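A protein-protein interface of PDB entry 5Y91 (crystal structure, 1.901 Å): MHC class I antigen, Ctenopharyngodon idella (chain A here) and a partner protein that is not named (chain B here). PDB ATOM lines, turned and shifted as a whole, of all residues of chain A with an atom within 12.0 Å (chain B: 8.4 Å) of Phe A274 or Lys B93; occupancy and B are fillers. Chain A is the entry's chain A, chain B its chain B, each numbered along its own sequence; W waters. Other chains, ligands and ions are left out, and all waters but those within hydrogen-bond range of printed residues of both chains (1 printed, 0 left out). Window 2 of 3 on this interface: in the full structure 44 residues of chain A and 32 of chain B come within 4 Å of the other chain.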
ATOM      1  N   LEU A 185     -17.825 -21.138  24.819  1.00  0.00           N
ATOM      2  CA  LEU A 185     -16.750 -22.019  25.254  1.00  0.00           C
ATOM      3  C   LEU A 185     -15.940 -22.447  24.038  1.00  0.00           C
ATOM      4  O   LEU A 185     -16.476 -23.053  23.110  1.00  0.00           O
ATOM      5  CB  LEU A 185     -17.311 -23.247  25.972  1.00  0.00           C
ATOM      6  CG  LEU A 185     -17.709 -23.071  27.434  1.00  0.00           C
ATOM      7  CD1 LEU A 185     -18.377 -24.329  27.968  1.00  0.00           C
ATOM      8  CD2 LEU A 185     -16.494 -22.714  28.274  1.00  0.00           C
ATOM      9  N   LEU A 186     -14.651 -22.125  24.050  1.00  0.00           N
ATOM     10  CA  LEU A 186     -13.773 -22.368  22.914  1.00  0.00           C
ATOM     11  C   LEU A 186     -12.772 -23.476  23.216  1.00  0.00           C
ATOM     12  O   LEU A 186     -12.304 -23.609  24.345  1.00  0.00           O
ATOM     13  CB  LEU A 186     -13.016 -21.088  22.555  1.00  0.00           C
ATOM     14  CG  LEU A 186     -13.712 -20.001  21.731  1.00  0.00           C
ATOM     15  CD1 LEU A 186     -15.198 -19.885  22.047  1.00  0.00           C
ATOM     16  CD2 LEU A 186     -13.005 -18.668  21.926  1.00  0.00           C
ATOM     17  N   GLN A 187     -12.443 -24.265  22.199  1.00  0.00           N
ATOM     18  CA  GLN A 187     -11.430 -25.303  22.337  1.00  0.00           C
ATOM     19  C   GLN A 187     -10.848 -25.644  20.972  1.00  0.00           C
ATOM     20  O   GLN A 187     -11.586 -25.952  20.039  1.00  0.00           O
ATOM     21  CB  GLN A 187     -12.026 -26.554  22.988  1.00  0.00           C
ATOM     22  CG  GLN A 187     -10.983 -27.556  23.452  1.00  0.00           C
ATOM     23  CD  GLN A 187     -11.591 -28.806  24.068  1.00  0.00           C
ATOM     24  OE1 GLN A 187     -12.666 -29.251  23.670  1.00  0.00           O
ATOM     25  NE2 GLN A 187     -10.895 -29.382  25.042  1.00  0.00           N
ATOM     26  N   LYS A 188      -9.528 -25.580  20.852  1.00  0.00           N
ATOM     27  CA  LYS A 188      -8.875 -25.904  19.590  1.00  0.00           C
ATOM     28  C   LYS A 188      -8.925 -27.404  19.341  1.00  0.00           C
ATOM     29  O   LYS A 188      -9.227 -27.851  18.235  1.00  0.00           O
ATOM     30  CB  LYS A 188      -7.421 -25.424  19.583  1.00  0.00           C
ATOM     31  CG  LYS A 188      -7.256 -23.915  19.693  1.00  0.00           C
ATOM     32  CD  LYS A 188      -5.806 -23.501  19.492  1.00  0.00           C
ATOM     33  CE  LYS A 188      -5.364 -23.684  18.044  1.00  0.00           C
ATOM     34  NZ  LYS A 188      -6.052 -22.735  17.117  1.00  0.00           N
ATOM     35  N   ASP A 189      -8.634 -28.172  20.388  1.00  0.00           N
ATOM     36  CA  ASP A 189      -8.549 -29.623  20.303  1.00  0.00           C
ATOM     37  C   ASP A 189      -9.255 -30.247  21.494  1.00  0.00           C
ATOM     38  O   ASP A 189      -9.255 -29.676  22.578  1.00  0.00           O
ATOM     39  CB  ASP A 189      -7.082 -30.056  20.308  1.00  0.00           C
ATOM     40  CG  ASP A 189      -6.728 -30.934  19.130  1.00  0.00           C
ATOM     41  OD1 ASP A 189      -7.308 -30.734  18.042  1.00  0.00           O
ATOM     42  OD2 ASP A 189      -5.867 -31.824  19.291  1.00  0.00           O
ATOM     43  N   PRO A 190      -9.855 -31.432  21.299  1.00  0.00           N
ATOM     44  CA  PRO A 190     -10.508 -32.148  22.401  1.00  0.00           C
ATOM     45  C   PRO A 190      -9.560 -32.363  23.578  1.00  0.00           C
ATOM     46  O   PRO A 190     -10.010 -32.616  24.697  1.00  0.00           O
ATOM     47  CB  PRO A 190     -10.873 -33.496  21.772  1.00  0.00           C
ATOM     48  CG  PRO A 190     -11.017 -33.197  20.321  1.00  0.00           C
ATOM     49  CD  PRO A 190      -9.989 -32.148  20.021  1.00  0.00           C
ATOM     50  N   SER A 192      -7.012 -30.018  24.089  1.00  0.00           N
ATOM     51  CA  SER A 192      -6.518 -28.680  24.398  1.00  0.00           C
ATOM     52  C   SER A 192      -7.273 -28.025  25.553  1.00  0.00           C
ATOM     53  O   SER A 192      -8.332 -28.501  25.955  1.00  0.00           O
ATOM     54  CB  SER A 192      -6.588 -27.793  23.153  1.00  0.00           C
ATOM     55  OG  SER A 192      -5.664 -28.233  22.175  1.00  0.00           O
ATOM     56  N   ILE A 270     -19.351 -26.368  23.817  1.00  0.00           N
ATOM     57  CA  ILE A 270     -18.029 -26.128  23.245  1.00  0.00           C
ATOM     58  C   ILE A 270     -18.042 -26.049  21.722  1.00  0.00           C
ATOM     59  O   ILE A 270     -18.579 -26.927  21.046  1.00  0.00           O
ATOM     60  CB  ILE A 270     -17.022 -27.205  23.686  1.00  0.00           C
ATOM     61  CG1 ILE A 270     -16.799 -27.127  25.197  1.00  0.00           C
ATOM     62  CG2 ILE A 270     -15.709 -27.043  22.942  1.00  0.00           C
ATOM     63  CD1 ILE A 270     -15.738 -28.070  25.702  1.00  0.00           C
ATOM     64  N   ILE A 271     -17.447 -24.987  21.190  1.00  0.00           N
ATOM     65  CA  ILE A 271     -17.320 -24.821  19.748  1.00  0.00           C
ATOM     66  C   ILE A 271     -15.852 -24.848  19.337  1.00  0.00           C
ATOM     67  O   ILE A 271     -14.964 -24.647  20.165  1.00  0.00           O
ATOM     68  CB  ILE A 271     -17.964 -23.511  19.260  1.00  0.00           C
ATOM     69  CG1 ILE A 271     -17.334 -22.309  19.969  1.00  0.00           C
ATOM     70  CG2 ILE A 271     -19.471 -23.542  19.483  1.00  0.00           C
ATOM     71  CD1 ILE A 271     -17.904 -20.973  19.524  1.00  0.00           C
ATOM     72  N   THR A 272     -15.605 -25.094  18.055  1.00  0.00           N
ATOM     73  CA  THR A 272     -14.245 -25.212  17.548  1.00  0.00           C
ATOM     74  C   THR A 272     -14.207 -25.087  16.028  1.00  0.00           C
ATOM     75  O   THR A 272     -15.207 -25.332  15.351  1.00  0.00           O
ATOM     76  CB  THR A 272     -13.630 -26.575  17.944  1.00  0.00           C
ATOM     77  OG1 THR A 272     -12.276 -26.659  17.476  1.00  0.00           O
ATOM     78  CG2 THR A 272     -14.436 -27.712  17.342  1.00  0.00           C
ATOM     79  N   ASN A 273     -13.056 -24.672  15.509  1.00  0.00           N
ATOM     80  CA  ASN A 273     -12.719 -24.867  14.107  1.00  0.00           C
ATOM     81  C   ASN A 273     -11.908 -26.162  14.063  1.00  0.00           C
ATOM     82  O   ASN A 273     -10.974 -26.334  14.852  1.00  0.00           O
ATOM     83  CB  ASN A 273     -11.871 -23.704  13.571  1.00  0.00           C
ATOM     84  CG  ASN A 273     -12.579 -22.352  13.657  1.00  0.00           C
ATOM     85  OD1 ASN A 273     -13.789 -22.247  13.459  1.00  0.00           O
ATOM     86  ND2 ASN A 273     -11.810 -21.307  13.935  1.00  0.00           N
ATOM     87  N   PHE A 274     -12.243 -27.080  13.163  1.00  0.00           N
ATOM     88  CA  PHE A 274     -13.276 -26.893  12.164  1.00  0.00           C
ATOM     89  C   PHE A 274     -14.472 -27.797  12.449  1.00  0.00           C
ATOM     90  O   PHE A 274     -15.460 -27.793  11.712  1.00  0.00           O
ATOM     91  CB  PHE A 274     -12.694 -27.219  10.791  1.00  0.00           C
ATOM     92  CG  PHE A 274     -11.366 -27.923  10.853  1.00  0.00           C
ATOM     93  CD1 PHE A 274     -11.298 -29.307  10.857  1.00  0.00           C
ATOM     94  CD2 PHE A 274     -10.189 -27.201  10.930  1.00  0.00           C
ATOM     95  CE1 PHE A 274     -10.078 -29.957  10.922  1.00  0.00           C
ATOM     96  CE2 PHE A 274      -8.967 -27.846  10.994  1.00  0.00           C
ATOM     97  CZ  PHE A 274      -8.912 -29.225  10.989  1.00  0.00           C
ATOM     98  N   ASP A 275     -14.375 -28.572  13.525  1.00  0.00           N
ATOM     99  CA  ASP A 275     -15.453 -29.466  13.933  1.00  0.00           C
ATOM    100  C   ASP A 275     -16.714 -28.694  14.308  1.00  0.00           C
ATOM    101  O   ASP A 275     -16.956 -27.594  13.810  1.00  0.00           O
ATOM    102  CB  ASP A 275     -15.017 -30.338  15.114  1.00  0.00           C
ATOM    103  CG  ASP A 275     -13.916 -31.318  14.746  1.00  0.00           C
ATOM    104  OD1 ASP A 275     -13.467 -32.068  15.640  1.00  0.00           O
ATOM    105  OD2 ASP A 275     -13.500 -31.340  13.569  1.00  0.00           O
ATOM    106  N   GLY B  34     -13.436 -16.489  16.917  1.00  0.00           N
ATOM    107  CA  GLY B  34     -12.956 -16.524  15.548  1.00  0.00           C
ATOM    108  C   GLY B  34     -13.434 -17.717  14.737  1.00  0.00           C
ATOM    109  O   GLY B  34     -12.621 -18.470  14.199  1.00  0.00           O
ATOM    110  N   GLU B  35     -14.750 -17.886  14.647  1.00  0.00           N
ATOM    111  CA  GLU B  35     -15.332 -18.953  13.841  1.00  0.00           C
ATOM    112  C   GLU B  35     -15.065 -18.696  12.365  1.00  0.00           C
ATOM    113  O   GLU B  35     -15.339 -17.609  11.861  1.00  0.00           O
ATOM    114  CB  GLU B  35     -16.844 -19.033  14.057  1.00  0.00           C
ATOM    115  CG  GLU B  35     -17.278 -19.264  15.490  1.00  0.00           C
ATOM    116  CD  GLU B  35     -18.790 -19.235  15.639  1.00  0.00           C
ATOM    117  OE1 GLU B  35     -19.495 -19.439  14.624  1.00  0.00           O
ATOM    118  OE2 GLU B  35     -19.276 -19.005  16.767  1.00  0.00           O
ATOM    119  N   TYR B  36     -14.544 -19.700  11.670  1.00  0.00           N
ATOM    120  CA  TYR B  36     -14.294 -19.567  10.241  1.00  0.00           C
ATOM    121  C   TYR B  36     -15.582 -19.240   9.494  1.00  0.00           C
ATOM    122  O   TYR B  36     -16.637 -19.803   9.786  1.00  0.00           O
ATOM    123  CB  TYR B  36     -13.668 -20.845   9.675  1.00  0.00           C
ATOM    124  CG  TYR B  36     -12.232 -21.061  10.093  1.00  0.00           C
ATOM    125  CD1 TYR B  36     -11.378 -19.984  10.294  1.00  0.00           C
ATOM    126  CD2 TYR B  36     -11.725 -22.341  10.267  1.00  0.00           C
ATOM    127  CE1 TYR B  36     -10.062 -20.176  10.670  1.00  0.00           C
ATOM    128  CE2 TYR B  36     -10.412 -22.543  10.641  1.00  0.00           C
ATOM    129  CZ  TYR B  36      -9.585 -21.459  10.841  1.00  0.00           C
ATOM    130  OH  TYR B  36      -8.276 -21.660  11.214  1.00  0.00           O
ATOM    131  N   GLY B  37     -15.489 -18.316   8.540  1.00  0.00           N
ATOM    132  CA  GLY B  37     -16.617 -17.966   7.695  1.00  0.00           C
ATOM    133  C   GLY B  37     -17.570 -16.936   8.273  1.00  0.00           C
ATOM    134  O   GLY B  37     -18.498 -16.497   7.592  1.00  0.00           O
ATOM    135  N   ASN B  61      -1.988 -12.450   5.729  1.00  0.00           N
ATOM    136  CA  ASN B  61      -0.931 -13.161   5.021  1.00  0.00           C
ATOM    137  C   ASN B  61       0.266 -12.256   4.727  1.00  0.00           C
ATOM    138  O   ASN B  61       0.866 -12.325   3.654  1.00  0.00           O
ATOM    139  CB  ASN B  61      -1.470 -13.786   3.731  1.00  0.00           C
ATOM    140  CG  ASN B  61      -2.548 -14.821   3.994  1.00  0.00           C
ATOM    141  OD1 ASN B  61      -2.438 -15.630   4.915  1.00  0.00           O
ATOM    142  ND2 ASN B  61      -3.600 -14.800   3.183  1.00  0.00           N
ATOM    143  N   LYS B  90     -13.082 -11.672   7.985  1.00  0.00           N
ATOM    144  CA  LYS B  90     -13.838 -12.910   7.910  1.00  0.00           C
ATOM    145  C   LYS B  90     -12.831 -14.045   7.813  1.00  0.00           C
ATOM    146  O   LYS B  90     -12.477 -14.473   6.716  1.00  0.00           O
ATOM    147  CB  LYS B  90     -14.744 -12.888   6.679  1.00  0.00           C
ATOM    148  CG  LYS B  90     -15.699 -14.065   6.556  1.00  0.00           C
ATOM    149  CD  LYS B  90     -16.523 -13.942   5.282  1.00  0.00           C
ATOM    150  CE  LYS B  90     -17.504 -15.088   5.131  1.00  0.00           C
ATOM    151  NZ  LYS B  90     -18.311 -14.960   3.886  1.00  0.00           N
ATOM    152  N   PRO B  91     -12.350 -14.519   8.968  1.00  0.00           N
ATOM    153  CA  PRO B  91     -11.264 -15.503   9.017  1.00  0.00           C
ATOM    154  C   PRO B  91     -11.622 -16.786   8.282  1.00  0.00           C
ATOM    155  O   PRO B  91     -12.736 -17.289   8.419  1.00  0.00           O
ATOM    156  CB  PRO B  91     -11.101 -15.776  10.517  1.00  0.00           C
ATOM    157  CG  PRO B  91     -12.385 -15.332  11.136  1.00  0.00           C
ATOM    158  CD  PRO B  91     -12.843 -14.175  10.311  1.00  0.00           C
ATOM    159  N   GLU B  92     -10.676 -17.297   7.499  1.00  0.00           N
ATOM    160  CA  GLU B  92     -10.852 -18.562   6.798  1.00  0.00           C
ATOM    161  C   GLU B  92      -9.641 -19.456   7.032  1.00  0.00           C
ATOM    162  O   GLU B  92      -8.566 -18.980   7.397  1.00  0.00           O
ATOM    163  CB  GLU B  92     -11.064 -18.335   5.299  1.00  0.00           C
ATOM    164  CG  GLU B  92     -12.287 -17.494   4.947  1.00  0.00           C
ATOM    165  CD  GLU B  92     -13.603 -18.208   5.204  1.00  0.00           C
ATOM    166  OE1 GLU B  92     -13.591 -19.311   5.788  1.00  0.00           O
ATOM    167  OE2 GLU B  92     -14.658 -17.660   4.820  1.00  0.00           O
ATOM    168  N   LYS B  93      -9.829 -20.752   6.811  1.00  0.00           N
ATOM    169  CA  LYS B  93      -8.830 -21.765   7.135  1.00  0.00           C
ATOM    170  C   LYS B  93      -7.409 -21.426   6.685  1.00  0.00           C
ATOM    171  O   LYS B  93      -6.444 -21.670   7.410  1.00  0.00           O
ATOM    172  CB  LYS B  93      -9.247 -23.114   6.545  1.00  0.00           C
ATOM    173  CG  LYS B  93      -9.237 -24.244   7.551  1.00  0.00           C
ATOM    174  CD  LYS B  93      -7.914 -24.288   8.296  1.00  0.00           C
ATOM    175  CE  LYS B  93      -7.978 -25.236   9.479  1.00  0.00           C
ATOM    176  NZ  LYS B  93      -6.733 -25.204  10.292  1.00  0.00           N
ATOM    177  N   SER B  94      -7.280 -20.866   5.490  1.00  0.00           N
ATOM    178  CA  SER B  94      -5.966 -20.685   4.881  1.00  0.00           C
ATOM    179  C   SER B  94      -5.179 -19.505   5.446  1.00  0.00           C
ATOM    180  O   SER B  94      -3.947 -19.520   5.459  1.00  0.00           O
ATOM    181  CB  SER B  94      -6.110 -20.521   3.365  1.00  0.00           C
ATOM    182  OG  SER B  94      -6.851 -21.589   2.803  1.00  0.00           O
ATOM    183  N   ASP B  95      -5.890 -18.490   5.922  1.00  0.00           N
ATOM    184  CA  ASP B  95      -5.283 -17.180   6.146  1.00  0.00           C
ATOM    185  C   ASP B  95      -4.696 -16.945   7.538  1.00  0.00           C
ATOM    186  O   ASP B  95      -5.215 -17.430   8.543  1.00  0.00           O
ATOM    187  CB  ASP B  95      -6.285 -16.081   5.790  1.00  0.00           C
ATOM    188  CG  ASP B  95      -6.745 -16.170   4.346  1.00  0.00           C
ATOM    189  OD1 ASP B  95      -5.888 -16.401   3.467  1.00  0.00           O
ATOM    190  OD2 ASP B  95      -7.956 -16.016   4.088  1.00  0.00           O
ATOM    191  N   GLU B  96      -3.602 -16.189   7.572  1.00  0.00           N
ATOM    192  CA  GLU B  96      -2.960 -15.789   8.816  1.00  0.00           C
ATOM    193  C   GLU B  96      -3.139 -14.293   9.036  1.00  0.00           C
ATOM    194  O   GLU B  96      -2.725 -13.483   8.207  1.00  0.00           O
ATOM    195  CB  GLU B  96      -1.465 -16.107   8.778  1.00  0.00           C
ATOM    196  CG  GLU B  96      -0.680 -15.471   9.922  1.00  0.00           C
ATOM    197  CD  GLU B  96       0.807 -15.374   9.634  1.00  0.00           C
ATOM    198  OE1 GLU B  96       1.540 -16.334   9.952  1.00  0.00           O
ATOM    199  OE2 GLU B  96       1.247 -14.334   9.097  1.00  0.00           O
ATOM    200  N   TYR B  97      -3.757 -13.929  10.154  1.00  0.00           N
ATOM    201  CA  TYR B  97      -3.918 -12.522  10.498  1.00  0.00           C
ATOM    202  C   TYR B  97      -2.971 -12.148  11.623  1.00  0.00           C
ATOM    203  O   TYR B  97      -2.741 -12.936  12.535  1.00  0.00           O
ATOM    204  CB  TYR B  97      -5.364 -12.217  10.882  1.00  0.00           C
ATOM    205  CG  TYR B  97      -6.323 -12.366   9.724  1.00  0.00           C
ATOM    206  CD1 TYR B  97      -6.576 -11.302   8.865  1.00  0.00           C
ATOM    207  CD2 TYR B  97      -6.961 -13.572   9.479  1.00  0.00           C
ATOM    208  CE1 TYR B  97      -7.446 -11.436   7.802  1.00  0.00           C
ATOM    209  CE2 TYR B  97      -7.829 -13.717   8.417  1.00  0.00           C
ATOM    210  CZ  TYR B  97      -8.067 -12.647   7.582  1.00  0.00           C
ATOM    211  OH  TYR B  97      -8.934 -12.784   6.525  1.00  0.00           O
ATOM    212  N   SER B 114      -7.015 -17.725  17.329  1.00  0.00           N
ATOM    213  CA  SER B 114      -8.466 -17.846  17.428  1.00  0.00           C
ATOM    214  C   SER B 114      -8.893 -18.597  18.682  1.00  0.00           C
ATOM    215  O   SER B 114     -10.009 -18.420  19.168  1.00  0.00           O
ATOM    216  CB  SER B 114      -9.030 -18.557  16.199  1.00  0.00           C
ATOM    217  OG  SER B 114      -8.680 -19.930  16.211  1.00  0.00           O
ATOM    218  N   MET B 116      -9.574 -21.540  18.630  1.00  0.00           N
ATOM    219  CA  MET B 116     -10.537 -22.508  18.115  1.00  0.00           C
ATOM    220  C   MET B 116      -9.889 -23.419  17.084  1.00  0.00           C
ATOM    221  O   MET B 116     -10.486 -24.412  16.668  1.00  0.00           O
ATOM    222  CB  MET B 116     -11.729 -21.795  17.478  1.00  0.00           C
ATOM    223  CG  MET B 116     -12.483 -20.880  18.417  1.00  0.00           C
ATOM    224  SD  MET B 116     -13.840 -20.038  17.588  1.00  0.00           S
ATOM    225  CE  MET B 116     -14.893 -21.412  17.130  1.00  0.00           C
ATOM    226  OXT MET B 116      -8.768 -23.174  16.634  1.00  0.00           O
HETATM  227  O   HOH W   1      -8.740 -22.377  14.014  1.00  0.00           O
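Met B116 touches Leu A186 (CG to CG, 3.6 Å).
Met B116 touches Gln A187.
Lys A188 touches Ser B114 (NZ to OG, 3.9 Å).
Ile A271 touches Glu B35 (CD1 to OE2, 3.7 Å).
Ile A271 touches Met B116 (CG1 to CE, 3.9 Å).
OD1 of Asn A273 touches CA of Glu B35, at 3.7 Å.
CE2 of Phe A274 touches CE of Lys B93, at 3.2 Å.
The backbone carbonyl oxygen of Leu A185 lies within hydrogen-bond range of the backbone NH of Ile A271, at 2.9 Å.
The side-chain amide nitrogen (NE2) of Gln A187 sits close to the backbone carbonyl oxygen (O) of Asp A189 (3.0 Å).
The side-chain amide nitrogen of Gln A187 is in hydrogen-bond range of the backbone carbonyl oxygen of Ser A192, 2.9 Å away.
N of Gln A187 sits at hydrogen-bond distance from O of Ile A271 (3.3 Å).
The side-chain sulfur of Met B116 is in hydrogen-bond range of the backbone NH of Gly B34, 3.6 Å away.
N of Glu B35 is in hydrogen-bond range of SD of Met B116 (3.8 Å).
Water W1 lies within hydrogen-bond range of OXT of Met B116, OH of Tyr B36, ND2 of Asn A273 and OG of Ser B114.
Of the 13 printed residues of chain A, 7 touch a printed residue of chain B.
Along chain A the printed residues that touch a printed residue of chain B span positions 186 to 274.
Of the 15 printed residues of chain B, 6 touch a printed residue of chain A.
Among the printed residues, 12 pairs touch across the chains.
Phe A274 touches just one residue of chain B: Lys B93 (3.2 Å).
Of chain A, only Phe A274 (3.2 Å) comes within 4 Å of Lys B93.
Tyr B36 touches one residue of chain A.
No residue of chain A comes within 4 Å of Glu B92.
No residue of chain A comes within 4 Å of Asp B95.
Printed residues of chain A within 4 Å of Glu B35: Ile A271 and Asn A273.
Printed residues of chain B within 4 Å of Gln A187: Met B116 (3.9 Å).
Of the printed residues of chain A, Gly B34 touches Asn A273.
Printed residues of chain A within 4 Å of Met B116: Leu A186, Gln A187, Lys A188, Ile A271, Thr A272 and Asn A273.
Printed residues of chain B within 4 Å of Asn A273: Gly B34, Glu B35, Tyr B36 and Met B116.
The nearest residue of chain B that does not touch Phe A274 is Tyr B36 (4.7 Å).
The side-chain amino group (NZ) of Lys A188 lies within salt-bridge range of the chain-end carboxylate (OXT) of Met B116, at 2.8 Å.
The side-chain hydroxyl (OG1) of Thr A272 lies within hydrogen-bond range of the chain-end carboxylate (O) of Met B116, at 3.0 Å.
ND2 of Asn A273 is in hydrogen-bond range of O of Gly B34.
N of Tyr B36 is in hydrogen-bond range of OD1 of Asn A273 (3.2 Å).
The chain-end carboxylate (O) of Met B116 sits at hydrogen-bond distance from the backbone NH (N) of Asn A273 (2.8 Å).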
